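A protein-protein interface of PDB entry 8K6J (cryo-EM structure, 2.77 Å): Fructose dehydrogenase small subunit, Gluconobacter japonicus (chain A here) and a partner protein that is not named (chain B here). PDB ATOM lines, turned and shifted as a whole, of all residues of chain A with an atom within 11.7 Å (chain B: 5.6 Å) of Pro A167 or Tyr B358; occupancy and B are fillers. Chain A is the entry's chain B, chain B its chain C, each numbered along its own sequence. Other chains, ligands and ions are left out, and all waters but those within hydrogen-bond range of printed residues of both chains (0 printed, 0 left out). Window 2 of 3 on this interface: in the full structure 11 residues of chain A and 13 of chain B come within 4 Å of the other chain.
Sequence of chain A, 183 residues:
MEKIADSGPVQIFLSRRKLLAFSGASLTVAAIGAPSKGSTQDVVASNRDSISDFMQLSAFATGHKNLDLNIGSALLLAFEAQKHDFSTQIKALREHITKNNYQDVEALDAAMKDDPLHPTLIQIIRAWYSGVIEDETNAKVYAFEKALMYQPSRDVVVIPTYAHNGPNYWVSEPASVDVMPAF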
ATOM      1  N   VAL A 158     -21.629  28.600  -7.452  1.00  0.00           N
ATOM      2  CA  VAL A 158     -23.061  28.454  -7.229  1.00  0.00           C
ATOM      3  C   VAL A 158     -23.787  28.495  -8.564  1.00  0.00           C
ATOM      4  O   VAL A 158     -23.583  29.411  -9.368  1.00  0.00           O
ATOM      5  CB  VAL A 158     -23.574  29.555  -6.291  1.00  0.00           C
ATOM      6  CG1 VAL A 158     -22.888  30.866  -6.604  1.00  0.00           C
ATOM      7  CG2 VAL A 158     -25.076  29.708  -6.426  1.00  0.00           C
ATOM      8  N   TYR A 162     -30.192  28.929  -7.744  1.00  0.00           N
ATOM      9  CA  TYR A 162     -30.299  27.997  -6.629  1.00  0.00           C
ATOM     10  C   TYR A 162     -29.167  28.219  -5.636  1.00  0.00           C
ATOM     11  O   TYR A 162     -28.000  28.325  -6.022  1.00  0.00           O
ATOM     12  CB  TYR A 162     -30.289  26.562  -7.144  1.00  0.00           C
ATOM     13  CG  TYR A 162     -31.479  26.252  -8.013  1.00  0.00           C
ATOM     14  CD1 TYR A 162     -31.468  26.548  -9.365  1.00  0.00           C
ATOM     15  CD2 TYR A 162     -32.620  25.683  -7.477  1.00  0.00           C
ATOM     16  CE1 TYR A 162     -32.555  26.275 -10.160  1.00  0.00           C
ATOM     17  CE2 TYR A 162     -33.712  25.405  -8.263  1.00  0.00           C
ATOM     18  CZ  TYR A 162     -33.674  25.704  -9.604  1.00  0.00           C
ATOM     19  OH  TYR A 162     -34.764  25.427 -10.394  1.00  0.00           O
ATOM     20  N   ALA A 163     -29.515  28.274  -4.356  1.00  0.00           N
ATOM     21  CA  ALA A 163     -28.559  28.663  -3.331  1.00  0.00           C
ATOM     22  C   ALA A 163     -27.598  27.530  -2.994  1.00  0.00           C
ATOM     23  O   ALA A 163     -27.939  26.347  -3.067  1.00  0.00           O
ATOM     24  CB  ALA A 163     -29.290  29.100  -2.066  1.00  0.00           C
ATOM     25  N   HIS A 164     -26.382  27.911  -2.618  1.00  0.00           N
ATOM     26  CA  HIS A 164     -25.435  26.996  -2.000  1.00  0.00           C
ATOM     27  C   HIS A 164     -25.784  26.873  -0.515  1.00  0.00           C
ATOM     28  O   HIS A 164     -26.817  27.366  -0.056  1.00  0.00           O
ATOM     29  CB  HIS A 164     -24.008  27.482  -2.226  1.00  0.00           C
ATOM     30  CG  HIS A 164     -23.107  26.463  -2.847  1.00  0.00           C
ATOM     31  ND1 HIS A 164     -21.883  26.129  -2.311  1.00  0.00           N
ATOM     32  CD2 HIS A 164     -23.246  25.711  -3.964  1.00  0.00           C
ATOM     33  CE1 HIS A 164     -21.309  25.211  -3.067  1.00  0.00           C
ATOM     34  NE2 HIS A 164     -22.115  24.940  -4.077  1.00  0.00           N
ATOM     35  N   ASN A 165     -24.918  26.236   0.265  1.00  0.00           N
ATOM     36  CA  ASN A 165     -25.246  25.914   1.651  1.00  0.00           C
ATOM     37  C   ASN A 165     -25.058  27.145   2.527  1.00  0.00           C
ATOM     38  O   ASN A 165     -23.948  27.452   2.962  1.00  0.00           O
ATOM     39  CB  ASN A 165     -24.394  24.755   2.152  1.00  0.00           C
ATOM     40  CG  ASN A 165     -22.930  24.932   1.837  1.00  0.00           C
ATOM     41  OD1 ASN A 165     -22.549  25.845   1.109  1.00  0.00           O
ATOM     42  ND2 ASN A 165     -22.096  24.061   2.388  1.00  0.00           N
ATOM     43  N   GLY A 166     -26.150  27.855   2.800  1.00  0.00           N
ATOM     44  CA  GLY A 166     -26.149  28.880   3.817  1.00  0.00           C
ATOM     45  C   GLY A 166     -25.768  30.253   3.310  1.00  0.00           C
ATOM     46  O   GLY A 166     -25.186  30.409   2.235  1.00  0.00           O
ATOM     47  N   PRO A 167     -26.090  31.284   4.095  1.00  0.00           N
ATOM     48  CA  PRO A 167     -25.859  32.665   3.658  1.00  0.00           C
ATOM     49  C   PRO A 167     -24.450  33.188   3.877  1.00  0.00           C
ATOM     50  O   PRO A 167     -24.227  34.386   3.678  1.00  0.00           O
ATOM     51  CB  PRO A 167     -26.865  33.463   4.506  1.00  0.00           C
ATOM     52  CG  PRO A 167     -27.812  32.458   5.052  1.00  0.00           C
ATOM     53  CD  PRO A 167     -26.997  31.232   5.247  1.00  0.00           C
ATOM     54  N   ASN A 168     -23.497  32.368   4.313  1.00  0.00           N
ATOM     55  CA  ASN A 168     -22.121  32.844   4.402  1.00  0.00           C
ATOM     56  C   ASN A 168     -21.123  31.758   4.025  1.00  0.00           C
ATOM     57  O   ASN A 168     -20.021  31.705   4.582  1.00  0.00           O
ATOM     58  CB  ASN A 168     -21.811  33.385   5.797  1.00  0.00           C
ATOM     59  CG  ASN A 168     -22.044  34.879   5.903  1.00  0.00           C
ATOM     60  OD1 ASN A 168     -21.967  35.600   4.911  1.00  0.00           O
ATOM     61  ND2 ASN A 168     -22.325  35.351   7.109  1.00  0.00           N
ATOM     62  N   TYR A 169     -21.486  30.884   3.087  1.00  0.00           N
ATOM     63  CA  TYR A 169     -20.616  29.764   2.749  1.00  0.00           C
ATOM     64  C   TYR A 169     -19.311  30.220   2.110  1.00  0.00           C
ATOM     65  O   TYR A 169     -18.300  29.517   2.212  1.00  0.00           O
ATOM     66  CB  TYR A 169     -21.344  28.797   1.818  1.00  0.00           C
ATOM     67  CG  TYR A 169     -21.615  29.355   0.440  1.00  0.00           C
ATOM     68  CD1 TYR A 169     -22.757  30.097   0.187  1.00  0.00           C
ATOM     69  CD2 TYR A 169     -20.735  29.131  -0.607  1.00  0.00           C
ATOM     70  CE1 TYR A 169     -23.009  30.606  -1.066  1.00  0.00           C
ATOM     71  CE2 TYR A 169     -20.980  29.637  -1.862  1.00  0.00           C
ATOM     72  CZ  TYR A 169     -22.118  30.374  -2.085  1.00  0.00           C
ATOM     73  OH  TYR A 169     -22.369  30.881  -3.337  1.00  0.00           O
ATOM     74  N   TRP A 170     -19.305  31.382   1.455  1.00  0.00           N
ATOM     75  CA  TRP A 170     -18.136  31.786   0.684  1.00  0.00           C
ATOM     76  C   TRP A 170     -16.949  32.173   1.554  1.00  0.00           C
ATOM     77  O   TRP A 170     -15.857  32.379   1.018  1.00  0.00           O
ATOM     78  CB  TRP A 170     -18.487  32.943  -0.249  1.00  0.00           C
ATOM     79  CG  TRP A 170     -19.195  34.075   0.406  1.00  0.00           C
ATOM     80  CD1 TRP A 170     -18.629  35.141   1.033  1.00  0.00           C
ATOM     81  CD2 TRP A 170     -20.608  34.265   0.490  1.00  0.00           C
ATOM     82  NE1 TRP A 170     -19.600  35.984   1.504  1.00  0.00           N
ATOM     83  CE2 TRP A 170     -20.827  35.467   1.183  1.00  0.00           C
ATOM     84  CE3 TRP A 170     -21.710  33.536   0.046  1.00  0.00           C
ATOM     85  CZ2 TRP A 170     -22.100  35.952   1.444  1.00  0.00           C
ATOM     86  CZ3 TRP A 170     -22.971  34.019   0.308  1.00  0.00           C
ATOM     87  CH2 TRP A 170     -23.157  35.216   0.994  1.00  0.00           C
ATOM     88  N   VAL A 171     -17.132  32.287   2.870  1.00  0.00           N
ATOM     89  CA  VAL A 171     -16.003  32.557   3.753  1.00  0.00           C
ATOM     90  C   VAL A 171     -15.001  31.411   3.710  1.00  0.00           C
ATOM     91  O   VAL A 171     -13.797  31.620   3.898  1.00  0.00           O
ATOM     92  CB  VAL A 171     -16.504  32.820   5.184  1.00  0.00           C
ATOM     93  CG1 VAL A 171     -15.375  33.333   6.057  1.00  0.00           C
ATOM     94  CG2 VAL A 171     -17.646  33.811   5.162  1.00  0.00           C
ATOM     95  N   SER A 172     -15.472  30.195   3.459  1.00  0.00           N
ATOM     96  CA  SER A 172     -14.595  29.037   3.403  1.00  0.00           C
ATOM     97  C   SER A 172     -13.762  29.046   2.127  1.00  0.00           C
ATOM     98  O   SER A 172     -14.162  29.601   1.100  1.00  0.00           O
ATOM     99  CB  SER A 172     -15.410  27.748   3.479  1.00  0.00           C
ATOM    100  OG  SER A 172     -16.050  27.482   2.245  1.00  0.00           O
ATOM    101  N   LYS B 257     -33.670  24.883  16.663  1.00  0.00           N
ATOM    102  CA  LYS B 257     -33.174  24.374  15.396  1.00  0.00           C
ATOM    103  C   LYS B 257     -32.704  22.941  15.578  1.00  0.00           C
ATOM    104  O   LYS B 257     -31.897  22.655  16.467  1.00  0.00           O
ATOM    105  CB  LYS B 257     -32.030  25.246  14.874  1.00  0.00           C
ATOM    106  CG  LYS B 257     -31.457  24.807  13.544  1.00  0.00           C
ATOM    107  CD  LYS B 257     -30.595  25.904  12.951  1.00  0.00           C
ATOM    108  CE  LYS B 257     -29.681  25.372  11.868  1.00  0.00           C
ATOM    109  NZ  LYS B 257     -29.017  26.480  11.131  1.00  0.00           N
ATOM    110  N   ARG B 262     -37.946  22.754  12.992  1.00  0.00           N
ATOM    111  CA  ARG B 262     -37.571  24.132  13.273  1.00  0.00           C
ATOM    112  C   ARG B 262     -38.738  24.836  13.944  1.00  0.00           C
ATOM    113  O   ARG B 262     -39.897  24.629  13.572  1.00  0.00           O
ATOM    114  CB  ARG B 262     -37.164  24.881  12.003  1.00  0.00           C
ATOM    115  CG  ARG B 262     -36.247  24.098  11.089  1.00  0.00           C
ATOM    116  CD  ARG B 262     -34.875  23.945  11.713  1.00  0.00           C
ATOM    117  NE  ARG B 262     -33.992  23.116  10.904  1.00  0.00           N
ATOM    118  CZ  ARG B 262     -32.997  23.586  10.166  1.00  0.00           C
ATOM    119  NH1 ARG B 262     -32.730  24.879  10.110  1.00  0.00           N
ATOM    120  NH2 ARG B 262     -32.248  22.737   9.470  1.00  0.00           N
ATOM    121  N   SER B 354     -30.393  22.926   2.293  1.00  0.00           N
ATOM    122  CA  SER B 354     -28.980  23.194   2.090  1.00  0.00           C
ATOM    123  C   SER B 354     -28.124  22.178   2.841  1.00  0.00           C
ATOM    124  O   SER B 354     -28.589  21.477   3.743  1.00  0.00           O
ATOM    125  CB  SER B 354     -28.635  24.611   2.540  1.00  0.00           C
ATOM    126  OG  SER B 354     -28.694  24.725   3.949  1.00  0.00           O
ATOM    127  N   ASP B 356     -25.488  22.733   4.814  1.00  0.00           N
ATOM    128  CA  ASP B 356     -25.119  23.132   6.165  1.00  0.00           C
ATOM    129  C   ASP B 356     -26.307  23.186   7.113  1.00  0.00           C
ATOM    130  O   ASP B 356     -26.123  23.502   8.292  1.00  0.00           O
ATOM    131  CB  ASP B 356     -24.415  24.490   6.143  1.00  0.00           C
ATOM    132  CG  ASP B 356     -25.310  25.599   5.643  1.00  0.00           C
ATOM    133  OD1 ASP B 356     -26.248  25.306   4.873  1.00  0.00           O
ATOM    134  OD2 ASP B 356     -25.075  26.767   6.018  1.00  0.00           O
ATOM    135  N   GLY B 357     -27.511  22.897   6.631  1.00  0.00           N
ATOM    136  CA  GLY B 357     -28.679  22.848   7.481  1.00  0.00           C
ATOM    137  C   GLY B 357     -29.323  24.182   7.770  1.00  0.00           C
ATOM    138  O   GLY B 357     -30.313  24.221   8.512  1.00  0.00           O
ATOM    139  N   TYR B 358     -28.796  25.277   7.220  1.00  0.00           N
ATOM    140  CA  TYR B 358     -29.420  26.578   7.434  1.00  0.00           C
ATOM    141  C   TYR B 358     -30.836  26.601   6.877  1.00  0.00           C
ATOM    142  O   TYR B 358     -31.754  27.128   7.515  1.00  0.00           O
ATOM    143  CB  TYR B 358     -28.574  27.678   6.800  1.00  0.00           C
ATOM    144  CG  TYR B 358     -29.001  29.074   7.184  1.00  0.00           C
ATOM    145  CD1 TYR B 358     -30.016  29.720   6.500  1.00  0.00           C
ATOM    146  CD2 TYR B 358     -28.390  29.744   8.231  1.00  0.00           C
ATOM    147  CE1 TYR B 358     -30.410  30.990   6.844  1.00  0.00           C
ATOM    148  CE2 TYR B 358     -28.780  31.018   8.583  1.00  0.00           C
ATOM    149  CZ  TYR B 358     -29.789  31.636   7.884  1.00  0.00           C
ATOM    150  OH  TYR B 358     -30.185  32.906   8.228  1.00  0.00           O
ATOM    151  N   TYR B 359     -31.032  26.035   5.689  1.00  0.00           N
ATOM    152  CA  TYR B 359     -32.361  25.906   5.117  1.00  0.00           C
ATOM    153  C   TYR B 359     -32.870  24.505   5.395  1.00  0.00           C
ATOM    154  O   TYR B 359     -32.277  23.535   4.900  1.00  0.00           O
ATOM    155  CB  TYR B 359     -32.332  26.187   3.620  1.00  0.00           C
ATOM    156  CG  TYR B 359     -31.889  27.593   3.321  1.00  0.00           C
ATOM    157  CD1 TYR B 359     -32.371  28.653   4.065  1.00  0.00           C
ATOM    158  CD2 TYR B 359     -30.977  27.862   2.314  1.00  0.00           C
ATOM    159  CE1 TYR B 359     -31.970  29.937   3.816  1.00  0.00           C
ATOM    160  CE2 TYR B 359     -30.570  29.152   2.054  1.00  0.00           C
ATOM    161  CZ  TYR B 359     -31.074  30.185   2.810  1.00  0.00           C
ATOM    162  OH  TYR B 359     -30.685  31.478   2.571  1.00  0.00           O
ATOM    163  N   PRO B 360     -33.938  24.344   6.167  1.00  0.00           N
ATOM    164  CA  PRO B 360     -34.313  23.011   6.639  1.00  0.00           C
ATOM    165  C   PRO B 360     -34.714  22.094   5.499  1.00  0.00           C
ATOM    166  O   PRO B 360     -35.256  22.526   4.480  1.00  0.00           O
ATOM    167  CB  PRO B 360     -35.497  23.287   7.567  1.00  0.00           C
ATOM    168  CG  PRO B 360     -36.078  24.543   7.053  1.00  0.00           C
ATOM    169  CD  PRO B 360     -34.930  25.362   6.547  1.00  0.00           C
ATOM    170  N   HIS B 391     -28.577  35.700  16.836  1.00  0.00           N
ATOM    171  CA  HIS B 391     -28.558  35.346  15.424  1.00  0.00           C
ATOM    172  C   HIS B 391     -29.968  34.964  14.998  1.00  0.00           C
ATOM    173  O   HIS B 391     -30.638  34.185  15.684  1.00  0.00           O
ATOM    174  CB  HIS B 391     -27.586  34.198  15.160  1.00  0.00           C
ATOM    175  CG  HIS B 391     -27.482  33.817  13.716  1.00  0.00           C
ATOM    176  ND1 HIS B 391     -27.468  34.749  12.701  1.00  0.00           N
ATOM    177  CD2 HIS B 391     -27.382  32.607  13.118  1.00  0.00           C
ATOM    178  CE1 HIS B 391     -27.369  34.129  11.539  1.00  0.00           C
ATOM    179  NE2 HIS B 391     -27.314  32.829  11.764  1.00  0.00           N
ATOM    180  N   GLU B 392     -30.412  35.509  13.871  1.00  0.00           N
ATOM    181  CA  GLU B 392     -31.801  35.427  13.442  1.00  0.00           C
ATOM    182  C   GLU B 392     -31.894  34.732  12.094  1.00  0.00           C
ATOM    183  O   GLU B 392     -31.199  35.120  11.150  1.00  0.00           O
ATOM    184  CB  GLU B 392     -32.401  36.832  13.350  1.00  0.00           C
ATOM    185  CG  GLU B 392     -33.889  36.886  13.096  1.00  0.00           C
ATOM    186  CD  GLU B 392     -34.363  38.291  12.785  1.00  0.00           C
ATOM    187  OE1 GLU B 392     -33.908  39.235  13.462  1.00  0.00           O
ATOM    188  OE2 GLU B 392     -35.189  38.456  11.865  1.00  0.00           O
ATOM    189  N   ILE B 393     -32.742  33.705  11.996  1.00  0.00           N
ATOM    190  CA  ILE B 393     -33.101  33.210  10.673  1.00  0.00           C
ATOM    191  C   ILE B 393     -34.347  33.974  10.267  1.00  0.00           C
ATOM    192  O   ILE B 393     -35.003  34.590  11.113  1.00  0.00           O
ATOM    193  CB  ILE B 393     -33.394  31.701  10.579  1.00  0.00           C
ATOM    194  CG1 ILE B 393     -32.835  30.855  11.722  1.00  0.00           C
ATOM    195  CG2 ILE B 393     -32.764  31.193   9.313  1.00  0.00           C
ATOM    196  CD1 ILE B 393     -31.333  30.954  11.909  1.00  0.00           C
ATOM    197  N   LEU B 394     -34.699  33.935   8.986  1.00  0.00           N
ATOM    198  CA  LEU B 394     -35.972  34.521   8.584  1.00  0.00           C
ATOM    199  C   LEU B 394     -36.438  33.907   7.277  1.00  0.00           C
ATOM    200  O   LEU B 394     -35.837  34.152   6.226  1.00  0.00           O
ATOM    201  CB  LEU B 394     -35.863  36.034   8.454  1.00  0.00           C
ATOM    202  CG  LEU B 394     -37.170  36.710   8.052  1.00  0.00           C
ATOM    203  CD1 LEU B 394     -37.512  37.811   9.037  1.00  0.00           C
ATOM    204  CD2 LEU B 394     -37.097  37.250   6.650  1.00  0.00           C
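The side-chain carboxylate of Asp B356 sits at hydrogen-bond distance from the backbone NH of Gly A166 (3.3 Å). O of Asn A165 sits close to OD2 of Asp B356 (3.3 Å).
N of Gly B357 sits at hydrogen-bond distance from OG of Ser B354 (3.5 Å). OG of Ser B354 lies within hydrogen-bond range of N of Tyr B358 (3.3 Å). OG of Ser B354 sits at hydrogen-bond distance from N of Tyr B359 (3.2 Å). The side-chain carboxylate (OD1) of Asp B356 sits close to the backbone NH (N) of Tyr B358. The side-chain amide oxygen of Asn A165 is in hydrogen-bond range of a ring nitrogen (ND1) of His A164 (3.5 Å). OG of Ser B354 is in hydrogen-bond range of OD1 of Asp B356 (2.7 Å).
Ser B354 touches Asn A165. CE1 of Tyr B358 touches CG of Pro A167, 3.5 Å away. Pro A167 touches Tyr B359.
Val A158 touches none of the printed residues of chain B. Ala A163 touches none of the printed residues of chain B. Of the printed residues of chain B, Asn A165 touches Ser B354 and Asp B356. Printed residues of chain B within 4 Å of Gly A166: Asp B356 (3.2 Å). Of chain B, only Tyr B358 and Tyr B359 come within 4 Å of Pro A167. Ser B354 touches one residue of chain A. Gly B357 touches none of the printed residues of chain A. Of the printed residues of chain A, Tyr B358 touches Pro A167 (3.5 Å). Of chain A, only Pro A167 (3.9 Å) comes within 4 Å of Tyr B359. No residue of chain A comes within 4 Å of Ile B393. The nearest residue of chain B that does not touch Pro A167 is Asp B356 (4.9 Å). The nearest residue of chain A that does not touch Tyr B358 is Gly A166 (4.03 Å). The nearest printed residue of chain B that does not touch Asn A165 is Tyr B358 (5.6 Å).
Of the 12 printed residues of chain B, 4 touch a printed residue of chain A. Printed residues of chain B that touch a printed residue of chain A: Ser B354, Asp B356, Tyr B358 and Tyr B359. Of the 12 printed residues of chain A, 3 touch a printed residue of chain B. Hydrophobic or aromatic side chains of chain A within 4 Å of the printed part of chain B: Pro A167. Among the printed residues, 5 pairs touch across the chains. Among the printed residues, no Asp or Glu carboxylate lies within 4 Å of a Lys or Arg side-chain nitrogen of the other chain.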
